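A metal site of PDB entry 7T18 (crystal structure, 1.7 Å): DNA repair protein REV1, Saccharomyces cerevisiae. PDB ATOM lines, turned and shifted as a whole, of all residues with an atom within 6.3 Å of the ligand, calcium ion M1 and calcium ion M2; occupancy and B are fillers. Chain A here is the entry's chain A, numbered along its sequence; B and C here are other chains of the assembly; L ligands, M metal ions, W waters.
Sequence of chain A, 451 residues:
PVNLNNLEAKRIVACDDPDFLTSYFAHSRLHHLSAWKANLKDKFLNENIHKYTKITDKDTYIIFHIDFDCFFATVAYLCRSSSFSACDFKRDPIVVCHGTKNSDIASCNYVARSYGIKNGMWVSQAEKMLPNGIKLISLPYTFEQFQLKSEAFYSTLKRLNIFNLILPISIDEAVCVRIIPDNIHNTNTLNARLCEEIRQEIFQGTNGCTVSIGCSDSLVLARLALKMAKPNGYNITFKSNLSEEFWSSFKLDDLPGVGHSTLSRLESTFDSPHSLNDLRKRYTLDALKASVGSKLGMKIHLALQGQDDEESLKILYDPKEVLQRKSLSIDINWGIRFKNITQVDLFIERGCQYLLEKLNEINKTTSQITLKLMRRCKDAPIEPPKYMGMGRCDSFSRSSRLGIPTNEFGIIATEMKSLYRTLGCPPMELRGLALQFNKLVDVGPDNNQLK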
ATOM      1  N   ARG A  29      -6.218 -16.093 -15.250  1.00  0.00           N
ATOM      2  CA  ARG A  29      -5.069 -16.342 -14.380  1.00  0.00           C
ATOM      3  C   ARG A  29      -3.817 -16.646 -15.192  1.00  0.00           C
ATOM      4  O   ARG A  29      -2.715 -16.212 -14.832  1.00  0.00           O
ATOM      5  CB  ARG A  29      -5.359 -17.493 -13.413  1.00  0.00           C
ATOM      6  CG  ARG A  29      -5.403 -18.885 -14.070  1.00  0.00           C
ATOM      7  CD  ARG A  29      -5.999 -19.887 -13.121  1.00  0.00           C
ATOM      8  NE  ARG A  29      -5.500 -21.239 -13.328  1.00  0.00           N
ATOM      9  CZ  ARG A  29      -6.024 -22.110 -14.182  1.00  0.00           C
ATOM     10  NH1 ARG A  29      -7.053 -21.745 -14.931  1.00  0.00           N
ATOM     11  NH2 ARG A  29      -5.519 -23.336 -14.289  1.00  0.00           N
ATOM     12  N   LEU A  30      -3.961 -17.383 -16.291  1.00  0.00           N
ATOM     13  CA  LEU A  30      -2.783 -17.778 -17.051  1.00  0.00           C
ATOM     14  C   LEU A  30      -2.181 -16.581 -17.779  1.00  0.00           C
ATOM     15  O   LEU A  30      -0.958 -16.479 -17.920  1.00  0.00           O
ATOM     16  CB  LEU A  30      -3.119 -18.921 -17.996  1.00  0.00           C
ATOM     17  CG  LEU A  30      -3.460 -20.251 -17.287  1.00  0.00           C
ATOM     18  CD1 LEU A  30      -4.012 -21.280 -18.260  1.00  0.00           C
ATOM     19  CD2 LEU A  30      -2.254 -20.792 -16.595  1.00  0.00           C
ATOM     20  N   LEU A  33      -0.216 -14.870 -15.075  1.00  0.00           N
ATOM     21  CA  LEU A  33       1.001 -15.686 -14.794  1.00  0.00           C
ATOM     22  C   LEU A  33       2.119 -15.313 -15.776  1.00  0.00           C
ATOM     23  O   LEU A  33       3.249 -15.078 -15.323  1.00  0.00           O
ATOM     24  CB  LEU A  33       0.644 -17.169 -14.903  1.00  0.00           C
ATOM     25  CG  LEU A  33       0.954 -18.015 -13.673  1.00  0.00           C
ATOM     26  CD1 LEU A  33       1.130 -19.484 -14.049  1.00  0.00           C
ATOM     27  CD2 LEU A  33       2.209 -17.503 -12.961  1.00  0.00           C
ATOM     28  N   TRP A  36       3.066 -11.292 -15.480  1.00  0.00           N
ATOM     29  CA  TRP A  36       3.899 -11.092 -14.309  1.00  0.00           C
ATOM     30  C   TRP A  36       5.327 -11.556 -14.540  1.00  0.00           C
ATOM     31  O   TRP A  36       6.280 -10.864 -14.178  1.00  0.00           O
ATOM     32  CB  TRP A  36       3.316 -11.856 -13.127  1.00  0.00           C
ATOM     33  CG  TRP A  36       2.067 -11.311 -12.588  1.00  0.00           C
ATOM     34  CD1 TRP A  36       1.680 -10.004 -12.528  1.00  0.00           C
ATOM     35  CD2 TRP A  36       1.018 -12.066 -11.981  1.00  0.00           C
ATOM     36  NE1 TRP A  36       0.449  -9.905 -11.924  1.00  0.00           N
ATOM     37  CE2 TRP A  36       0.030 -11.164 -11.573  1.00  0.00           C
ATOM     38  CE3 TRP A  36       0.835 -13.437 -11.719  1.00  0.00           C
ATOM     39  CZ2 TRP A  36      -1.138 -11.577 -10.935  1.00  0.00           C
ATOM     40  CZ3 TRP A  36      -0.314 -13.842 -11.089  1.00  0.00           C
ATOM     41  CH2 TRP A  36      -1.290 -12.915 -10.711  1.00  0.00           C
ATOM     42  N   ASP A  67       9.360 -20.378  -2.395  1.00  0.00           N
ATOM     43  CA  ASP A  67       8.093 -20.396  -3.116  1.00  0.00           C
ATOM     44  C   ASP A  67       6.938 -20.270  -2.122  1.00  0.00           C
ATOM     45  O   ASP A  67       6.950 -20.922  -1.072  1.00  0.00           O
ATOM     46  CB  ASP A  67       7.982 -21.690  -3.945  1.00  0.00           C
ATOM     47  CG  ASP A  67       6.599 -21.906  -4.528  1.00  0.00           C
ATOM     48  OD1 ASP A  67       5.776 -22.549  -3.863  1.00  0.00           O
ATOM     49  OD2 ASP A  67       6.344 -21.419  -5.643  1.00  0.00           O
ATOM     50  N   PHE A  68       5.958 -19.416  -2.438  1.00  0.00           N
ATOM     51  CA  PHE A  68       4.768 -19.282  -1.594  1.00  0.00           C
ATOM     52  C   PHE A  68       3.970 -20.589  -1.575  1.00  0.00           C
ATOM     53  O   PHE A  68       3.707 -21.184  -2.625  1.00  0.00           O
ATOM     54  CB  PHE A  68       3.823 -18.202  -2.150  1.00  0.00           C
ATOM     55  CG  PHE A  68       4.188 -16.771  -1.841  1.00  0.00           C
ATOM     56  CD1 PHE A  68       5.214 -16.135  -2.509  1.00  0.00           C
ATOM     57  CD2 PHE A  68       3.406 -16.029  -0.972  1.00  0.00           C
ATOM     58  CE1 PHE A  68       5.505 -14.786  -2.290  1.00  0.00           C
ATOM     59  CE2 PHE A  68       3.669 -14.677  -0.742  1.00  0.00           C
ATOM     60  CZ  PHE A  68       4.724 -14.059  -1.387  1.00  0.00           C
ATOM     61  N   ASP A  69       3.517 -20.975  -0.399  1.00  0.00           N
ATOM     62  CA  ASP A  69       2.575 -22.102  -0.293  1.00  0.00           C
ATOM     63  C   ASP A  69       1.201 -21.628  -0.790  1.00  0.00           C
ATOM     64  O   ASP A  69       0.768 -20.615  -0.335  1.00  0.00           O
ATOM     65  CB  ASP A  69       2.426 -22.566   1.164  1.00  0.00           C
ATOM     66  CG  ASP A  69       3.765 -22.933   1.769  1.00  0.00           C
ATOM     67  OD1 ASP A  69       4.492 -23.622   1.109  1.00  0.00           O
ATOM     68  OD2 ASP A  69       4.032 -22.497   2.839  1.00  0.00           O
ATOM     69  N   CYS A  70       0.533 -22.479  -1.547  1.00  0.00           N
ATOM     70  CA  CYS A  70      -0.776 -22.264  -2.207  1.00  0.00           C
ATOM     71  C   CYS A  70      -1.029 -20.772  -2.432  1.00  0.00           C
ATOM     72  O   CYS A  70      -1.910 -20.252  -1.851  1.00  0.00           O
ATOM     73  CB  CYS A  70      -1.905 -22.955  -1.459  1.00  0.00           C
ATOM     74  SG  CYS A  70      -1.900 -22.636   0.328  1.00  0.00           S
ATOM     75  N   PHE A  71      -0.197 -20.169  -3.289  1.00  0.00           N
ATOM     76  CA  PHE A  71      -0.173 -18.715  -3.370  1.00  0.00           C
ATOM     77  C   PHE A  71      -1.537 -18.033  -3.498  1.00  0.00           C
ATOM     78  O   PHE A  71      -1.916 -17.217  -2.658  1.00  0.00           O
ATOM     79  CB  PHE A  71       0.725 -18.322  -4.539  1.00  0.00           C
ATOM     80  CG  PHE A  71       0.910 -16.856  -4.706  1.00  0.00           C
ATOM     81  CD1 PHE A  71       1.291 -16.070  -3.642  1.00  0.00           C
ATOM     82  CD2 PHE A  71       0.681 -16.256  -5.945  1.00  0.00           C
ATOM     83  CE1 PHE A  71       1.473 -14.713  -3.793  1.00  0.00           C
ATOM     84  CE2 PHE A  71       0.841 -14.888  -6.100  1.00  0.00           C
ATOM     85  CZ  PHE A  71       1.244 -14.123  -5.031  1.00  0.00           C
ATOM     86  N   PHE A  72      -2.296 -18.332  -4.566  1.00  0.00           N
ATOM     87  CA  PHE A  72      -3.570 -17.630  -4.744  1.00  0.00           C
ATOM     88  C   PHE A  72      -4.519 -17.922  -3.590  1.00  0.00           C
ATOM     89  O   PHE A  72      -5.279 -17.036  -3.173  1.00  0.00           O
ATOM     90  CB  PHE A  72      -4.255 -18.027  -6.044  1.00  0.00           C
ATOM     91  CG  PHE A  72      -3.701 -17.393  -7.295  1.00  0.00           C
ATOM     92  CD1 PHE A  72      -2.468 -16.761  -7.339  1.00  0.00           C
ATOM     93  CD2 PHE A  72      -4.459 -17.465  -8.470  1.00  0.00           C
ATOM     94  CE1 PHE A  72      -1.993 -16.216  -8.524  1.00  0.00           C
ATOM     95  CE2 PHE A  72      -3.996 -16.910  -9.662  1.00  0.00           C
ATOM     96  CZ  PHE A  72      -2.748 -16.306  -9.687  1.00  0.00           C
ATOM     97  N   ALA A  73      -4.546 -19.162  -3.094  1.00  0.00           N
ATOM     98  CA  ALA A  73      -5.476 -19.473  -1.999  1.00  0.00           C
ATOM     99  C   ALA A  73      -5.105 -18.708  -0.734  1.00  0.00           C
ATOM    100  O   ALA A  73      -5.981 -18.174  -0.059  1.00  0.00           O
ATOM    101  CB  ALA A  73      -5.510 -20.981  -1.734  1.00  0.00           C
ATOM    102  N   ALA A 106      -7.617 -22.559  -9.433  1.00  0.00           N
ATOM    103  CA  ALA A 106      -6.314 -21.917  -9.604  1.00  0.00           C
ATOM    104  C   ALA A 106      -5.355 -22.317  -8.497  1.00  0.00           C
ATOM    105  O   ALA A 106      -4.158 -22.524  -8.748  1.00  0.00           O
ATOM    106  CB  ALA A 106      -6.498 -20.401  -9.654  1.00  0.00           C
ATOM    107  N   SER A 107      -5.862 -22.421  -7.274  1.00  0.00           N
ATOM    108  CA  SER A 107      -5.070 -22.776  -6.107  1.00  0.00           C
ATOM    109  C   SER A 107      -6.011 -23.372  -5.088  1.00  0.00           C
ATOM    110  O   SER A 107      -7.165 -22.953  -4.971  1.00  0.00           O
ATOM    111  CB  SER A 107      -4.370 -21.537  -5.525  1.00  0.00           C
ATOM    112  OG  SER A 107      -3.453 -21.875  -4.486  1.00  0.00           O
ATOM    113  N   CYS A 108      -5.518 -24.360  -4.356  1.00  0.00           N
ATOM    114  CA  CYS A 108      -6.291 -24.897  -3.248  1.00  0.00           C
ATOM    115  C   CYS A 108      -5.358 -25.009  -2.052  1.00  0.00           C
ATOM    116  O   CYS A 108      -4.160 -25.224  -2.215  1.00  0.00           O
ATOM    117  CB  CYS A 108      -6.895 -26.263  -3.580  1.00  0.00           C
ATOM    118  SG  CYS A 108      -5.669 -27.469  -4.138  1.00  0.00           S
ATOM    119  N   TYR A 110      -3.989 -26.561   1.708  1.00  0.00           N
ATOM    120  CA  TYR A 110      -3.518 -27.909   1.990  1.00  0.00           C
ATOM    121  C   TYR A 110      -4.569 -28.751   2.696  1.00  0.00           C
ATOM    122  O   TYR A 110      -4.476 -29.983   2.666  1.00  0.00           O
ATOM    123  CB  TYR A 110      -2.188 -27.833   2.775  1.00  0.00           C
ATOM    124  CG  TYR A 110      -1.039 -27.589   1.820  1.00  0.00           C
ATOM    125  CD1 TYR A 110      -0.826 -26.333   1.270  1.00  0.00           C
ATOM    126  CD2 TYR A 110      -0.194 -28.615   1.432  1.00  0.00           C
ATOM    127  CE1 TYR A 110       0.207 -26.109   0.352  1.00  0.00           C
ATOM    128  CE2 TYR A 110       0.855 -28.399   0.531  1.00  0.00           C
ATOM    129  CZ  TYR A 110       1.040 -27.151  -0.007  1.00  0.00           C
ATOM    130  OH  TYR A 110       2.058 -26.924  -0.908  1.00  0.00           O
ATOM    131  N   ARG A 113      -6.134 -30.228  -0.254  1.00  0.00           N
ATOM    132  CA  ARG A 113      -5.237 -31.222  -0.820  1.00  0.00           C
ATOM    133  C   ARG A 113      -5.217 -32.509  -0.021  1.00  0.00           C
ATOM    134  O   ARG A 113      -4.901 -33.564  -0.575  1.00  0.00           O
ATOM    135  CB  ARG A 113      -3.819 -30.646  -0.929  1.00  0.00           C
ATOM    136  CG  ARG A 113      -3.726 -29.458  -1.889  1.00  0.00           C
ATOM    137  CD  ARG A 113      -2.320 -28.868  -1.975  1.00  0.00           C
ATOM    138  NE  ARG A 113      -2.366 -27.558  -2.625  1.00  0.00           N
ATOM    139  CZ  ARG A 113      -1.346 -26.975  -3.240  1.00  0.00           C
ATOM    140  NH1 ARG A 113      -0.166 -27.587  -3.298  1.00  0.00           N
ATOM    141  NH2 ARG A 113      -1.510 -25.780  -3.806  1.00  0.00           N
ATOM    142  N   ASN A 119      -4.441 -28.315  -7.685  1.00  0.00           N
ATOM    143  CA  ASN A 119      -4.519 -27.186  -8.601  1.00  0.00           C
ATOM    144  C   ASN A 119      -4.833 -27.690 -10.001  1.00  0.00           C
ATOM    145  O   ASN A 119      -4.292 -28.706 -10.455  1.00  0.00           O
ATOM    146  CB  ASN A 119      -3.195 -26.413  -8.636  1.00  0.00           C
ATOM    147  CG  ASN A 119      -2.927 -25.633  -7.364  1.00  0.00           C
ATOM    148  OD1 ASN A 119      -3.712 -25.670  -6.430  1.00  0.00           O
ATOM    149  ND2 ASN A 119      -1.799 -24.916  -7.335  1.00  0.00           N
ATOM    150  N   TYR A 141     -10.787 -14.526  -7.215  1.00  0.00           N
ATOM    151  CA  TYR A 141      -9.453 -14.006  -7.446  1.00  0.00           C
ATOM    152  C   TYR A 141      -9.303 -12.584  -6.910  1.00  0.00           C
ATOM    153  O   TYR A 141     -10.235 -11.778  -6.923  1.00  0.00           O
ATOM    154  CB  TYR A 141      -9.143 -13.987  -8.938  1.00  0.00           C
ATOM    155  CG  TYR A 141      -9.094 -15.326  -9.618  1.00  0.00           C
ATOM    156  CD1 TYR A 141     -10.253 -15.921 -10.118  1.00  0.00           C
ATOM    157  CD2 TYR A 141      -7.890 -15.998  -9.797  1.00  0.00           C
ATOM    158  CE1 TYR A 141     -10.213 -17.143 -10.768  1.00  0.00           C
ATOM    159  CE2 TYR A 141      -7.841 -17.221 -10.450  1.00  0.00           C
ATOM    160  CZ  TYR A 141      -8.995 -17.775 -10.946  1.00  0.00           C
ATOM    161  OH  TYR A 141      -8.928 -18.999 -11.606  1.00  0.00           O
ATOM    162  N   ILE A 169      11.561 -16.535 -10.748  1.00  0.00           N
ATOM    163  CA  ILE A 169      10.986 -17.664 -11.449  1.00  0.00           C
ATOM    164  C   ILE A 169       9.534 -17.391 -11.823  1.00  0.00           C
ATOM    165  O   ILE A 169       9.103 -17.697 -12.933  1.00  0.00           O
ATOM    166  CB  ILE A 169      11.091 -18.946 -10.598  1.00  0.00           C
ATOM    167  CG1 ILE A 169      12.547 -19.269 -10.285  1.00  0.00           C
ATOM    168  CG2 ILE A 169      10.407 -20.112 -11.294  1.00  0.00           C
ATOM    169  CD1 ILE A 169      13.362 -19.623 -11.524  1.00  0.00           C
ATOM    170  N   SER A 170       8.784 -16.802 -10.891  1.00  0.00           N
ATOM    171  CA  SER A 170       7.384 -16.502 -11.137  1.00  0.00           C
ATOM    172  C   SER A 170       6.927 -15.481 -10.099  1.00  0.00           C
ATOM    173  O   SER A 170       7.723 -14.990  -9.289  1.00  0.00           O
ATOM    174  CB  SER A 170       6.533 -17.770 -11.069  1.00  0.00           C
ATOM    175  OG  SER A 170       6.193 -18.034  -9.738  1.00  0.00           O
ATOM    176  N   ILE A 171       5.645 -15.146 -10.158  1.00  0.00           N
ATOM    177  CA  ILE A 171       5.032 -14.198  -9.232  1.00  0.00           C
ATOM    178  C   ILE A 171       5.307 -14.595  -7.779  1.00  0.00           C
ATOM    179  O   ILE A 171       5.461 -13.730  -6.908  1.00  0.00           O
ATOM    180  CB  ILE A 171       3.516 -14.104  -9.534  1.00  0.00           C
ATOM    181  CG1 ILE A 171       2.852 -13.031  -8.660  1.00  0.00           C
ATOM    182  CG2 ILE A 171       2.808 -15.457  -9.327  1.00  0.00           C
ATOM    183  CD1 ILE A 171       3.090 -11.638  -9.174  1.00  0.00           C
ATOM    184  N   ASP A 172       5.393 -15.901  -7.503  1.00  0.00           N
ATOM    185  CA  ASP A 172       5.503 -16.375  -6.125  1.00  0.00           C
ATOM    186  C   ASP A 172       6.749 -17.227  -5.873  1.00  0.00           C
ATOM    187  O   ASP A 172       6.792 -17.970  -4.887  1.00  0.00           O
ATOM    188  CB  ASP A 172       4.243 -17.165  -5.723  1.00  0.00           C
ATOM    189  CG  ASP A 172       4.265 -18.598  -6.228  1.00  0.00           C
ATOM    190  OD1 ASP A 172       4.790 -18.830  -7.326  1.00  0.00           O
ATOM    191  OD2 ASP A 172       3.766 -19.498  -5.527  1.00  0.00           O
ATOM    192  N   GLU A 173       7.778 -17.124  -6.717  1.00  0.00           N
ATOM    193  CA  GLU A 173       8.856 -18.094  -6.621  1.00  0.00           C
ATOM    194  C   GLU A 173      10.150 -17.472  -7.121  1.00  0.00           C
ATOM    195  O   GLU A 173      10.156 -16.832  -8.177  1.00  0.00           O
ATOM    196  CB  GLU A 173       8.519 -19.349  -7.431  1.00  0.00           C
ATOM    197  CG  GLU A 173       9.541 -20.454  -7.368  1.00  0.00           C
ATOM    198  CD  GLU A 173       9.088 -21.655  -8.184  1.00  0.00           C
ATOM    199  OE1 GLU A 173       9.897 -22.585  -8.408  1.00  0.00           O
ATOM    200  OE2 GLU A 173       7.909 -21.660  -8.594  1.00  0.00           O
ATOM    201  N   LYS A 230       7.341 -28.580   1.706  1.00  0.00           N
ATOM    202  CA  LYS A 230       5.997 -28.021   1.771  1.00  0.00           C
ATOM    203  C   LYS A 230       5.078 -28.861   2.652  1.00  0.00           C
ATOM    204  O   LYS A 230       5.234 -30.089   2.727  1.00  0.00           O
ATOM    205  CB  LYS A 230       5.399 -27.932   0.358  1.00  0.00           C
ATOM    206  CG  LYS A 230       5.957 -26.766  -0.447  1.00  0.00           C
ATOM    207  CD  LYS A 230       5.453 -26.762  -1.874  1.00  0.00           C
ATOM    208  CE  LYS A 230       5.699 -25.401  -2.529  1.00  0.00           C
ATOM    209  NZ  LYS A 230       5.099 -24.254  -1.755  1.00  0.00           N
ATOM    210  P    DG B  12       9.703 -23.453 -13.612  1.00  0.00           P
ATOM    211  OP1  DG B  12      11.022 -22.766 -13.807  1.00  0.00           O
ATOM    212  OP2  DG B  12       9.600 -24.543 -12.673  1.00  0.00           O
ATOM    213  O5'  DG B  12       8.668 -22.359 -13.147  1.00  0.00           O
ATOM    214  C5'  DG B  12       7.669 -22.604 -12.164  1.00  0.00           C
ATOM    215  C4'  DG B  12       6.583 -21.598 -12.426  1.00  0.00           C
ATOM    216  O4'  DG B  12       6.211 -21.763 -13.806  1.00  0.00           O
ATOM    217  C3'  DG B  12       5.294 -21.731 -11.637  1.00  0.00           C
ATOM    218  O3'  DG B  12       5.327 -20.946 -10.446  1.00  0.00           O
ATOM    219  C2'  DG B  12       4.280 -21.155 -12.594  1.00  0.00           C
ATOM    220  C1'  DG B  12       4.928 -21.304 -13.980  1.00  0.00           C
ATOM    221  N9   DG B  12       4.205 -22.239 -14.833  1.00  0.00           N
ATOM    222  C8   DG B  12       3.792 -23.518 -14.547  1.00  0.00           C
ATOM    223  N7   DG B  12       2.986 -24.002 -15.441  1.00  0.00           N
ATOM    224  C5   DG B  12       2.786 -22.954 -16.319  1.00  0.00           C
ATOM    225  C6   DG B  12       1.974 -22.869 -17.474  1.00  0.00           C
ATOM    226  O6   DG B  12       1.289 -23.735 -17.993  1.00  0.00           O
ATOM    227  N1   DG B  12       2.085 -21.620 -18.091  1.00  0.00           N
ATOM    228  C2   DG B  12       2.826 -20.579 -17.607  1.00  0.00           C
ATOM    229  N2   DG B  12       2.771 -19.446 -18.294  1.00  0.00           N
ATOM    230  N3   DG B  12       3.578 -20.643 -16.529  1.00  0.00           N
ATOM    231  C4   DG B  12       3.539 -21.861 -15.955  1.00  0.00           C
ATOM    232  P    DC C   5      -5.510 -19.768 -23.384  1.00  0.00           P
ATOM    233  OP1  DC C   5      -6.714 -19.076 -23.881  1.00  0.00           O
ATOM    234  OP2  DC C   5      -4.796 -20.704 -24.275  1.00  0.00           O
ATOM    235  O5'  DC C   5      -4.401 -18.738 -22.892  1.00  0.00           O
ATOM    236  C5'  DC C   5      -4.759 -17.676 -22.029  1.00  0.00           C
ATOM    237  C4'  DC C   5      -3.539 -16.908 -21.578  1.00  0.00           C
ATOM    238  O4'  DC C   5      -2.717 -17.736 -20.726  1.00  0.00           O
ATOM    239  C3'  DC C   5      -2.614 -16.447 -22.691  1.00  0.00           C
ATOM    240  O3'  DC C   5      -2.003 -15.260 -22.272  1.00  0.00           O
ATOM    241  C2'  DC C   5      -1.596 -17.588 -22.796  1.00  0.00           C
ATOM    242  C1'  DC C   5      -1.460 -18.000 -21.339  1.00  0.00           C
ATOM    243  N1   DC C   5      -1.179 -19.442 -21.111  1.00  0.00           N
ATOM    244  C2   DC C   5      -0.065 -19.810 -20.363  1.00  0.00           C
ATOM    245  O2   DC C   5       0.698 -18.922 -19.953  1.00  0.00           O
ATOM    246  N3   DC C   5       0.138 -21.111 -20.090  1.00  0.00           N
ATOM    247  C4   DC C   5      -0.707 -22.022 -20.541  1.00  0.00           C
ATOM    248  N4   DC C   5      -0.464 -23.292 -20.256  1.00  0.00           N
ATOM    249  C5   DC C   5      -1.870 -21.674 -21.299  1.00  0.00           C
ATOM    250  C6   DC C   5      -2.063 -20.379 -21.542  1.00  0.00           C
HETATM  251  P1  LIG L   1       2.257 -22.840  -7.949  1.00  0.00           P
HETATM  252  O1  LIG L   1       3.433 -22.440  -7.191  1.00  0.00           O
HETATM  253  O2  LIG L   1       2.468 -23.913  -8.915  1.00  0.00           O
HETATM  254  O3  LIG L   1       1.105 -23.344  -6.968  1.00  0.00           O
HETATM  255  P2  LIG L   1       0.607 -22.946  -5.502  1.00  0.00           P
HETATM  256  O4  LIG L   1       1.491 -21.918  -5.008  1.00  0.00           O
HETATM  257  O5  LIG L   1      -0.906 -22.621  -5.544  1.00  0.00           O
HETATM  258  O6  LIG L   1       0.794 -24.256  -4.626  1.00  0.00           O
HETATM  259  P3  LIG L   1       2.128 -24.896  -4.025  1.00  0.00           P
HETATM  260  O7  LIG L   1       3.273 -24.107  -4.587  1.00  0.00           O
HETATM  261  O8  LIG L   1       2.063 -24.784  -2.485  1.00  0.00           O
HETATM  262  O9  LIG L   1       2.124 -26.376  -4.448  1.00  0.00           O
HETATM  263  O10 LIG L   1       1.653 -21.588  -8.696  1.00  0.00           O
HETATM  264  C1  LIG L   1       1.592 -20.291  -8.092  1.00  0.00           C
HETATM  265  C2  LIG L   1       0.262 -19.658  -8.400  1.00  0.00           C
HETATM  266  O11 LIG L   1       0.187 -19.454  -9.819  1.00  0.00           O
HETATM  267  C3  LIG L   1      -0.940 -20.529  -8.053  1.00  0.00           C
HETATM  268  O12 LIG L   1      -1.410 -20.274  -6.731  1.00  0.00           O
HETATM  269  C4  LIG L   1      -1.964 -20.158  -9.098  1.00  0.00           C
HETATM  270  C5  LIG L   1      -1.126 -19.727 -10.292  1.00  0.00           C
HETATM  271  N1  LIG L   1      -1.034 -20.765 -11.323  1.00  0.00           N
HETATM  272  C6  LIG L   1      -2.036 -20.809 -12.298  1.00  0.00           C
HETATM  273  O13 LIG L   1      -2.944 -19.998 -12.278  1.00  0.00           O
HETATM  274  N2  LIG L   1      -1.978 -21.781 -13.293  1.00  0.00           N
HETATM  275  C7  LIG L   1      -0.968 -22.649 -13.204  1.00  0.00           C
HETATM  276  O14 LIG L   1      -0.951 -23.510 -14.079  1.00  0.00           O
HETATM  277  C8  LIG L   1       0.065 -22.669 -12.244  1.00  0.00           C
HETATM  278  C9  LIG L   1       1.179 -23.685 -12.242  1.00  0.00           C
HETATM  279  C10 LIG L   1       0.027 -21.714 -11.222  1.00  0.00           C
HETATM  280 CA    CA M   1       3.824 -21.783  -4.898  1.00  0.00          CA
HETATM  281 CA    CA M   2       5.464 -21.076  -7.988  1.00  0.00          CA
HETATM  282  O   HOH W   1      -3.859 -22.816 -11.429  1.00  0.00           O
HETATM  283  O   HOH W   2      -2.607 -25.839 -12.559  1.00  0.00           O
HETATM  284  O   HOH W   3       0.242 -25.421  -9.321  1.00  0.00           O
HETATM  285  O   HOH W   4       0.928 -27.345  -6.833  1.00  0.00           O
HETATM  286  O   HOH W   5      -0.619 -25.223 -16.653  1.00  0.00           O
HETATM  287  O   HOH W   6       4.122 -28.236  -4.549  1.00  0.00           O
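CD2 of Leu 30 touches N2 of the ligand, at 3.5 Å.
Leu 33 touches the ligand.
CA of Asp 69 touches O8 of the ligand, 3.5 Å away.
O of Ala 106 touches C4 of the ligand, 3.2 Å away.
Hydrophobic or aromatic side chains that line the ligand: Leu 30, Leu 33, Phe 71, Phe 72 and Tyr 110.
OG of Ser 170 touches calcium ion M2, at 3.6 Å.
Within 4 Å of calcium ion M2: Asp 67, Ser 170, Asp 172, Glu 173 and DG 12 of chain B.
OD1 of Asp 172 is bound to calcium ion M2 (2.4 Å).
O3' of DG 12 of chain B is bound to calcium ion M2, 2.5 Å away.
OD2 of Asp 67 is bound to calcium ion M2 (2.5 Å).
O1 of the ligand binds calcium ion M2 (2.6 Å).
OE2 of Glu 173 is bound to calcium ion M2 (2.6 Å).
Calcium ion M2 has five donor atoms within binding distance.
Of the 26 residues printed, 3 come within 4 Å of calcium ion M1.
The nearest printed residue that does not touch calcium ion M1 is Lys 230 (4.2 Å).
The side-chain carboxylate of Asp 67 sits close to the side-chain amino group of Lys 230 (2.8 Å).
The backbone carbonyl oxygen (O) of Phe 68 lies close to the side-chain amino group (NZ) of Lys 230.
The backbone NH (N) of Asp 172 sits close to the side-chain hydroxyl (OG) of Ser 170 (3.2 Å).
The guanidinium group (NH1) of Arg 113 is in hydrogen-bond range of the side-chain hydroxyl (OH) of Tyr 110, 3.3 Å away.
The guanidinium group (NH2) of Arg 113 is in hydrogen-bond range of the side-chain amide oxygen (OD1) of Asn 119 (3.4 Å).
The backbone carbonyl oxygen (O) of Cys 70 sits close to the side-chain hydroxyl (OG) of Ser 107, at 3.5 Å.
OG of Ser 107 lies within hydrogen-bond range of N of Ala 73 (3.2 Å).
The side-chain carboxylate of Asp 69 is in salt-bridge range of the side-chain amino group of Lys 230 (3.0 Å).
The side-chain carboxylate (OD1) of Asp 67 is bound to calcium ion M1 (2.3 Å).
An oxygen (O4) of the ligand is bound to calcium ion M1, at 2.3 Å.
O of Phe 68 binds calcium ion M1, 2.4 Å away.
The side-chain carboxylate (OD2) of Asp 172 is bound to calcium ion M1.
Calcium ion M1 is bound by O7 of the ligand.
Calcium ion M1 is bound by O1 of the ligand (2.4 Å).
The side-chain carboxylate (OD2) of Asp 67 is bound to calcium ion M1.
Calcium ion M1 has seven donor atoms within binding distance.
O8 of the ligand sits at hydrogen-bond distance from OH of Tyr 110 (2.7 Å).
An oxygen (O9) of the ligand lies within salt-bridge range of the guanidinium group (NH1) of Arg 113.
OG of Ser 107 is in hydrogen-bond range of O5 of the ligand.
The backbone NH (N) of Cys 70 sits at hydrogen-bond distance from an oxygen (O8) of the ligand, 2.9 Å away.
N of Phe 71 is in hydrogen-bond range of O5 of the ligand (3.4 Å).
O13 of the ligand is in hydrogen-bond range of NE of Arg 29 (3.0 Å).
N of Phe 72 lies within hydrogen-bond range of O12 of the ligand (3.0 Å).
ND2 of Asn 119 is in hydrogen-bond range of O5 of the ligand.
NZ of Lys 230 lies within salt-bridge range of O8 of the ligand (3.2 Å).
Water W3 lies within hydrogen-bond range of O2 of the ligand and ND2 of Asn 119.
Water W1 lies within hydrogen-bond range of O of Ala 106, N2 of the ligand and NE of Arg 29.
Water W5 lies within hydrogen-bond range of O6 of DG 12 of chain B (2.8 Å) and an oxygen (O14) of the ligand (3.1 Å).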
